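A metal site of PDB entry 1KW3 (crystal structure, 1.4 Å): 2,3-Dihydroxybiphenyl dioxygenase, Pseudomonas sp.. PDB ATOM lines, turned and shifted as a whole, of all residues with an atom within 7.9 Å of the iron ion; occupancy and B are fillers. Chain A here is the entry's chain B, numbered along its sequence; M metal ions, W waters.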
ATOM      1  N   HIS A 145     -25.885  30.273 -10.145  1.00  0.00           N
ATOM      2  CA  HIS A 145     -25.845  29.518 -11.397  1.00  0.00           C
ATOM      3  C   HIS A 145     -27.233  29.112 -11.840  1.00  0.00           C
ATOM      4  O   HIS A 145     -28.201  29.257 -11.118  1.00  0.00           O
ATOM      5  CB  HIS A 145     -24.912  28.276 -11.283  1.00  0.00           C
ATOM      6  CG  HIS A 145     -25.414  27.162 -10.415  1.00  0.00           C
ATOM      7  ND1 HIS A 145     -24.684  26.677  -9.355  1.00  0.00           N
ATOM      8  CD2 HIS A 145     -26.508  26.356 -10.497  1.00  0.00           C
ATOM      9  CE1 HIS A 145     -25.329  25.665  -8.790  1.00  0.00           C
ATOM     10  NE2 HIS A 145     -26.437  25.450  -9.476  1.00  0.00           N
ATOM     11  N   PHE A 146     -27.319  28.635 -13.076  1.00  0.00           N
ATOM     12  CA  PHE A 146     -28.544  27.995 -13.543  1.00  0.00           C
ATOM     13  C   PHE A 146     -28.221  26.836 -14.447  1.00  0.00           C
ATOM     14  O   PHE A 146     -27.119  26.754 -15.014  1.00  0.00           O
ATOM     15  CB  PHE A 146     -29.556  28.959 -14.195  1.00  0.00           C
ATOM     16  CG  PHE A 146     -29.066  29.654 -15.438  1.00  0.00           C
ATOM     17  CD1 PHE A 146     -29.267  29.107 -16.693  1.00  0.00           C
ATOM     18  CD2 PHE A 146     -28.497  30.901 -15.378  1.00  0.00           C
ATOM     19  CE1 PHE A 146     -28.860  29.757 -17.835  1.00  0.00           C
ATOM     20  CE2 PHE A 146     -28.076  31.558 -16.526  1.00  0.00           C
ATOM     21  CZ  PHE A 146     -28.258  30.981 -17.760  1.00  0.00           C
ATOM     22  N   VAL A 147     -29.154  25.900 -14.533  1.00  0.00           N
ATOM     23  CA  VAL A 147     -29.030  24.755 -15.422  1.00  0.00           C
ATOM     24  C   VAL A 147     -29.909  25.034 -16.635  1.00  0.00           C
ATOM     25  O   VAL A 147     -31.137  25.133 -16.521  1.00  0.00           O
ATOM     26  CB  VAL A 147     -29.453  23.460 -14.753  1.00  0.00           C
ATOM     27  CG1 VAL A 147     -29.442  22.304 -15.758  1.00  0.00           C
ATOM     28  CG2 VAL A 147     -28.527  23.175 -13.584  1.00  0.00           C
ATOM     29  N   PHE A 186     -21.034  20.953 -16.838  1.00  0.00           N
ATOM     30  CA  PHE A 186     -21.001  22.060 -15.872  1.00  0.00           C
ATOM     31  C   PHE A 186     -19.900  23.025 -16.263  1.00  0.00           C
ATOM     32  O   PHE A 186     -18.750  22.596 -16.346  1.00  0.00           O
ATOM     33  CB  PHE A 186     -20.791  21.481 -14.461  1.00  0.00           C
ATOM     34  CG  PHE A 186     -21.938  20.643 -13.994  1.00  0.00           C
ATOM     35  CD1 PHE A 186     -22.073  19.325 -14.399  1.00  0.00           C
ATOM     36  CD2 PHE A 186     -22.912  21.209 -13.196  1.00  0.00           C
ATOM     37  CE1 PHE A 186     -23.159  18.585 -13.990  1.00  0.00           C
ATOM     38  CE2 PHE A 186     -23.985  20.475 -12.785  1.00  0.00           C
ATOM     39  CZ  PHE A 186     -24.117  19.166 -13.189  1.00  0.00           C
ATOM     40  N   HIS A 194     -19.693  26.061 -11.111  1.00  0.00           N
ATOM     41  CA  HIS A 194     -20.340  26.343 -12.371  1.00  0.00           C
ATOM     42  C   HIS A 194     -21.254  27.553 -12.260  1.00  0.00           C
ATOM     43  O   HIS A 194     -21.805  27.845 -11.197  1.00  0.00           O
ATOM     44  CB  HIS A 194     -21.080  25.136 -12.951  1.00  0.00           C
ATOM     45  CG  HIS A 194     -22.165  24.585 -12.092  1.00  0.00           C
ATOM     46  ND1 HIS A 194     -21.899  23.797 -10.991  1.00  0.00           N
ATOM     47  CD2 HIS A 194     -23.517  24.612 -12.214  1.00  0.00           C
ATOM     48  CE1 HIS A 194     -23.037  23.389 -10.454  1.00  0.00           C
ATOM     49  NE2 HIS A 194     -24.035  23.864 -11.176  1.00  0.00           N
ATOM     50  N   ALA A 197     -24.859  25.226 -16.366  1.00  0.00           N
ATOM     51  CA  ALA A 197     -24.713  23.817 -16.717  1.00  0.00           C
ATOM     52  C   ALA A 197     -25.649  23.600 -17.892  1.00  0.00           C
ATOM     53  O   ALA A 197     -26.664  24.278 -18.022  1.00  0.00           O
ATOM     54  CB  ALA A 197     -25.055  22.906 -15.571  1.00  0.00           C
ATOM     55  N   HIS A 208     -33.834  24.373 -15.685  1.00  0.00           N
ATOM     56  CA  HIS A 208     -34.339  23.448 -14.685  1.00  0.00           C
ATOM     57  C   HIS A 208     -34.403  24.149 -13.320  1.00  0.00           C
ATOM     58  O   HIS A 208     -35.366  24.016 -12.587  1.00  0.00           O
ATOM     59  CB  HIS A 208     -33.453  22.205 -14.610  1.00  0.00           C
ATOM     60  CG  HIS A 208     -33.784  21.331 -13.458  1.00  0.00           C
ATOM     61  ND1 HIS A 208     -33.242  21.515 -12.208  1.00  0.00           N
ATOM     62  CD2 HIS A 208     -34.590  20.254 -13.360  1.00  0.00           C
ATOM     63  CE1 HIS A 208     -33.734  20.614 -11.376  1.00  0.00           C
ATOM     64  NE2 HIS A 208     -34.548  19.826 -12.058  1.00  0.00           N
ATOM     65  N   HIS A 209     -33.342  24.879 -12.977  1.00  0.00           N
ATOM     66  CA  HIS A 209     -33.300  25.621 -11.731  1.00  0.00           C
ATOM     67  C   HIS A 209     -32.263  26.733 -11.811  1.00  0.00           C
ATOM     68  O   HIS A 209     -31.430  26.774 -12.712  1.00  0.00           O
ATOM     69  CB  HIS A 209     -32.973  24.713 -10.518  1.00  0.00           C
ATOM     70  CG  HIS A 209     -31.547  24.229 -10.442  1.00  0.00           C
ATOM     71  ND1 HIS A 209     -31.150  23.034 -11.008  1.00  0.00           N
ATOM     72  CD2 HIS A 209     -30.467  24.710  -9.784  1.00  0.00           C
ATOM     73  CE1 HIS A 209     -29.872  22.823 -10.725  1.00  0.00           C
ATOM     74  NE2 HIS A 209     -29.432  23.828  -9.989  1.00  0.00           N
ATOM     75  N   PHE A 210     -32.392  27.659 -10.864  1.00  0.00           N
ATOM     76  CA  PHE A 210     -31.340  28.633 -10.578  1.00  0.00           C
ATOM     77  C   PHE A 210     -30.972  28.409  -9.109  1.00  0.00           C
ATOM     78  O   PHE A 210     -31.799  27.931  -8.325  1.00  0.00           O
ATOM     79  CB  PHE A 210     -31.735  30.090 -10.842  1.00  0.00           C
ATOM     80  CG  PHE A 210     -32.760  30.660  -9.911  1.00  0.00           C
ATOM     81  CD1 PHE A 210     -32.401  31.540  -8.917  1.00  0.00           C
ATOM     82  CD2 PHE A 210     -34.090  30.346 -10.056  1.00  0.00           C
ATOM     83  CE1 PHE A 210     -33.356  32.083  -8.078  1.00  0.00           C
ATOM     84  CE2 PHE A 210     -35.045  30.889  -9.217  1.00  0.00           C
ATOM     85  CZ  PHE A 210     -34.675  31.743  -8.213  1.00  0.00           C
ATOM     86  N   MET A 211     -29.728  28.748  -8.773  1.00  0.00           N
ATOM     87  CA  MET A 211     -29.193  28.518  -7.436  1.00  0.00           C
ATOM     88  C   MET A 211     -28.656  29.800  -6.825  1.00  0.00           C
ATOM     89  O   MET A 211     -27.976  30.567  -7.503  1.00  0.00           O
ATOM     90  CB  MET A 211     -28.043  27.520  -7.530  1.00  0.00           C
ATOM     91  CG  MET A 211     -27.401  27.123  -6.201  1.00  0.00           C
ATOM     92  SD  MET A 211     -26.048  28.199  -5.662  1.00  0.00           S
ATOM     93  CE  MET A 211     -25.457  27.318  -4.252  1.00  0.00           C
ATOM     94  N   LEU A 212     -28.995  29.995  -5.548  1.00  0.00           N
ATOM     95  CA  LEU A 212     -28.421  31.063  -4.728  1.00  0.00           C
ATOM     96  C   LEU A 212     -27.630  30.402  -3.604  1.00  0.00           C
ATOM     97  O   LEU A 212     -28.036  29.357  -3.069  1.00  0.00           O
ATOM     98  CB  LEU A 212     -29.484  31.975  -4.146  1.00  0.00           C
ATOM     99  CG  LEU A 212     -30.314  32.726  -5.175  1.00  0.00           C
ATOM    100  CD1 LEU A 212     -31.493  33.392  -4.488  1.00  0.00           C
ATOM    101  CD2 LEU A 212     -29.511  33.760  -5.963  1.00  0.00           C
ATOM    102  N   HIS A 240     -23.988  17.849  -3.458  1.00  0.00           N
ATOM    103  CA  HIS A 240     -23.667  17.398  -4.807  1.00  0.00           C
ATOM    104  C   HIS A 240     -22.274  16.794  -4.904  1.00  0.00           C
ATOM    105  O   HIS A 240     -21.361  17.177  -4.186  1.00  0.00           O
ATOM    106  CB  HIS A 240     -23.813  18.560  -5.773  1.00  0.00           C
ATOM    107  CG  HIS A 240     -25.234  18.889  -6.132  1.00  0.00           C
ATOM    108  ND1 HIS A 240     -26.028  18.032  -6.878  1.00  0.00           N
ATOM    109  CD2 HIS A 240     -25.984  19.985  -5.879  1.00  0.00           C
ATOM    110  CE1 HIS A 240     -27.213  18.612  -7.072  1.00  0.00           C
ATOM    111  NE2 HIS A 240     -27.205  19.789  -6.482  1.00  0.00           N
ATOM    112  N   ASN A 242     -20.103  16.990  -7.529  1.00  0.00           N
ATOM    113  CA  ASN A 242     -19.098  17.755  -8.257  1.00  0.00           C
ATOM    114  C   ASN A 242     -18.725  19.077  -7.602  1.00  0.00           C
ATOM    115  O   ASN A 242     -17.543  19.311  -7.350  1.00  0.00           O
ATOM    116  CB  ASN A 242     -19.442  17.903  -9.761  1.00  0.00           C
ATOM    117  CG  ASN A 242     -20.767  18.578 -10.022  1.00  0.00           C
ATOM    118  OD1 ASN A 242     -21.616  18.713  -9.136  1.00  0.00           O
ATOM    119  ND2 ASN A 242     -20.964  19.011 -11.272  1.00  0.00           N
ATOM    120  N   ASP A 243     -19.689  19.948  -7.323  1.00  0.00           N
ATOM    121  CA  ASP A 243     -19.365  21.221  -6.661  1.00  0.00           C
ATOM    122  C   ASP A 243     -19.468  21.106  -5.147  1.00  0.00           C
ATOM    123  O   ASP A 243     -18.972  21.974  -4.446  1.00  0.00           O
ATOM    124  CB  ASP A 243     -20.189  22.396  -7.202  1.00  0.00           C
ATOM    125  CG  ASP A 243     -21.625  22.327  -6.849  1.00  0.00           C
ATOM    126  OD1 ASP A 243     -22.323  23.350  -7.015  1.00  0.00           O
ATOM    127  OD2 ASP A 243     -22.169  21.306  -6.409  1.00  0.00           O
ATOM    128  N   THR A 245     -21.904  21.584  -3.390  1.00  0.00           N
ATOM    129  CA  THR A 245     -22.938  22.448  -2.817  1.00  0.00           C
ATOM    130  C   THR A 245     -23.849  21.604  -1.906  1.00  0.00           C
ATOM    131  O   THR A 245     -24.352  20.555  -2.321  1.00  0.00           O
ATOM    132  CB  THR A 245     -23.802  23.054  -3.930  1.00  0.00           C
ATOM    133  OG1 THR A 245     -23.070  24.080  -4.610  1.00  0.00           O
ATOM    134  CG2 THR A 245     -25.010  23.760  -3.377  1.00  0.00           C
ATOM    135  N   SER A 247     -27.326  21.698  -0.379  1.00  0.00           N
ATOM    136  CA  SER A 247     -28.520  22.435  -0.741  1.00  0.00           C
ATOM    137  C   SER A 247     -29.772  21.617  -0.650  1.00  0.00           C
ATOM    138  O   SER A 247     -29.724  20.399  -0.456  1.00  0.00           O
ATOM    139  CB  SER A 247     -28.423  22.890  -2.199  1.00  0.00           C
ATOM    140  OG  SER A 247     -28.312  21.746  -3.071  1.00  0.00           O
ATOM    141  N   TYR A 249     -33.765  21.720  -2.866  1.00  0.00           N
ATOM    142  CA  TYR A 249     -34.484  22.267  -4.008  1.00  0.00           C
ATOM    143  C   TYR A 249     -35.938  22.492  -3.616  1.00  0.00           C
ATOM    144  O   TYR A 249     -36.496  21.789  -2.776  1.00  0.00           O
ATOM    145  CB  TYR A 249     -34.401  21.311  -5.202  1.00  0.00           C
ATOM    146  CG  TYR A 249     -33.035  21.217  -5.853  1.00  0.00           C
ATOM    147  CD1 TYR A 249     -32.764  21.843  -7.054  1.00  0.00           C
ATOM    148  CD2 TYR A 249     -31.985  20.514  -5.248  1.00  0.00           C
ATOM    149  CE1 TYR A 249     -31.521  21.747  -7.666  1.00  0.00           C
ATOM    150  CE2 TYR A 249     -30.738  20.437  -5.847  1.00  0.00           C
ATOM    151  CZ  TYR A 249     -30.519  21.066  -7.047  1.00  0.00           C
ATOM    152  OH  TYR A 249     -29.304  21.028  -7.700  1.00  0.00           O
ATOM    153  N   VAL A 259     -35.895  26.324  -7.542  1.00  0.00           N
ATOM    154  CA  VAL A 259     -34.796  27.064  -6.945  1.00  0.00           C
ATOM    155  C   VAL A 259     -33.971  26.071  -6.107  1.00  0.00           C
ATOM    156  O   VAL A 259     -34.507  25.109  -5.525  1.00  0.00           O
ATOM    157  CB  VAL A 259     -35.264  28.226  -6.057  1.00  0.00           C
ATOM    158  CG1 VAL A 259     -36.005  27.727  -4.851  1.00  0.00           C
ATOM    159  CG2 VAL A 259     -34.072  29.106  -5.642  1.00  0.00           C
ATOM    160  N   GLU A 260     -32.669  26.291  -6.110  1.00  0.00           N
ATOM    161  CA  GLU A 260     -31.749  25.572  -5.245  1.00  0.00           C
ATOM    162  C   GLU A 260     -31.157  26.601  -4.283  1.00  0.00           C
ATOM    163  O   GLU A 260     -30.704  27.646  -4.707  1.00  0.00           O
ATOM    164  CB  GLU A 260     -30.661  24.916  -6.082  1.00  0.00           C
ATOM    165  CG  GLU A 260     -29.644  24.145  -5.265  1.00  0.00           C
ATOM    166  CD  GLU A 260     -28.489  23.661  -6.111  1.00  0.00           C
ATOM    167  OE1 GLU A 260     -28.357  24.108  -7.265  1.00  0.00           O
ATOM    168  OE2 GLU A 260     -27.689  22.833  -5.587  1.00  0.00           O
ATOM    169  N   PHE A 261     -31.173  26.287  -2.989  1.00  0.00           N
ATOM    170  CA  PHE A 261     -30.699  27.188  -1.940  1.00  0.00           C
ATOM    171  C   PHE A 261     -29.596  26.408  -1.221  1.00  0.00           C
ATOM    172  O   PHE A 261     -29.865  25.355  -0.629  1.00  0.00           O
ATOM    173  CB  PHE A 261     -31.856  27.535  -1.028  1.00  0.00           C
ATOM    174  CG  PHE A 261     -31.596  28.675  -0.086  1.00  0.00           C
ATOM    175  CD1 PHE A 261     -32.226  29.903  -0.267  1.00  0.00           C
ATOM    176  CD2 PHE A 261     -30.777  28.518   1.006  1.00  0.00           C
ATOM    177  CE1 PHE A 261     -32.021  30.943   0.612  1.00  0.00           C
ATOM    178  CE2 PHE A 261     -30.560  29.556   1.877  1.00  0.00           C
ATOM    179  CZ  PHE A 261     -31.178  30.775   1.666  1.00  0.00           C
ATOM    180  N   HIS A 285     -30.461  14.653  -0.895  1.00  0.00           N
ATOM    181  CA  HIS A 285     -31.220  15.099  -2.057  1.00  0.00           C
ATOM    182  C   HIS A 285     -32.315  14.143  -2.503  1.00  0.00           C
ATOM    183  O   HIS A 285     -32.720  14.169  -3.663  1.00  0.00           O
ATOM    184  CB  HIS A 285     -30.306  15.385  -3.243  1.00  0.00           C
ATOM    185  CG  HIS A 285     -29.590  16.694  -3.179  1.00  0.00           C
ATOM    186  ND1 HIS A 285     -28.448  16.923  -3.909  1.00  0.00           N
ATOM    187  CD2 HIS A 285     -29.836  17.848  -2.506  1.00  0.00           C
ATOM    188  CE1 HIS A 285     -28.024  18.155  -3.693  1.00  0.00           C
ATOM    189  NE2 HIS A 285     -28.843  18.739  -2.834  1.00  0.00           N
HETATM  190 FE    FE M   1     -27.515  23.680  -9.045  1.00  0.00          FE
HETATM  191  O   HOH W   1     -25.979  22.836  -7.626  1.00  0.00           O
HETATM  192  O   HOH W   2     -26.567  22.546 -10.636  1.00  0.00           O
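A ring nitrogen (ND1) of His 145 lies close to a ring nitrogen (NE2) of His 194, 3.4 Å away. The side-chain carboxylate of Glu 260 sits close to the side-chain hydroxyl of Tyr 249, 3.2 Å away. O of His 145 sits at hydrogen-bond distance from N of Met 211. OE2 of Glu 260 lies within hydrogen-bond range of OG of Ser 247 (2.8 Å). The backbone carbonyl oxygen of Phe 210 sits at hydrogen-bond distance from the backbone NH of Glu 260 (2.9 Å). The side-chain carboxylate of Glu 260 sits at hydrogen-bond distance from a ring nitrogen (NE2) of His 240 (3.2 Å). O of Glu 260 lies within hydrogen-bond range of N of Leu 212 (3.0 Å). OH of Tyr 249 sits at hydrogen-bond distance from NE2 of His 240 (2.7 Å).
Residues that only touch the iron ion: Tyr 249. Four residues have an atom within 4 Å of the iron ion: His 145, His 209, Tyr 249 and Glu 260.
The iron ion is bound by the side-chain carboxylate of Glu 260 (2.0 Å), a ring nitrogen (NE2) of His 145 (2.1 Å), a ring nitrogen (NE2) of His 209 (2.1 Å), water W2 (2.2 Å) and water W1 (2.3 Å).
Water W1 bridges OE2 of Glu 260 (2.7 Å) and NE2 of His 240 (3.5 Å).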
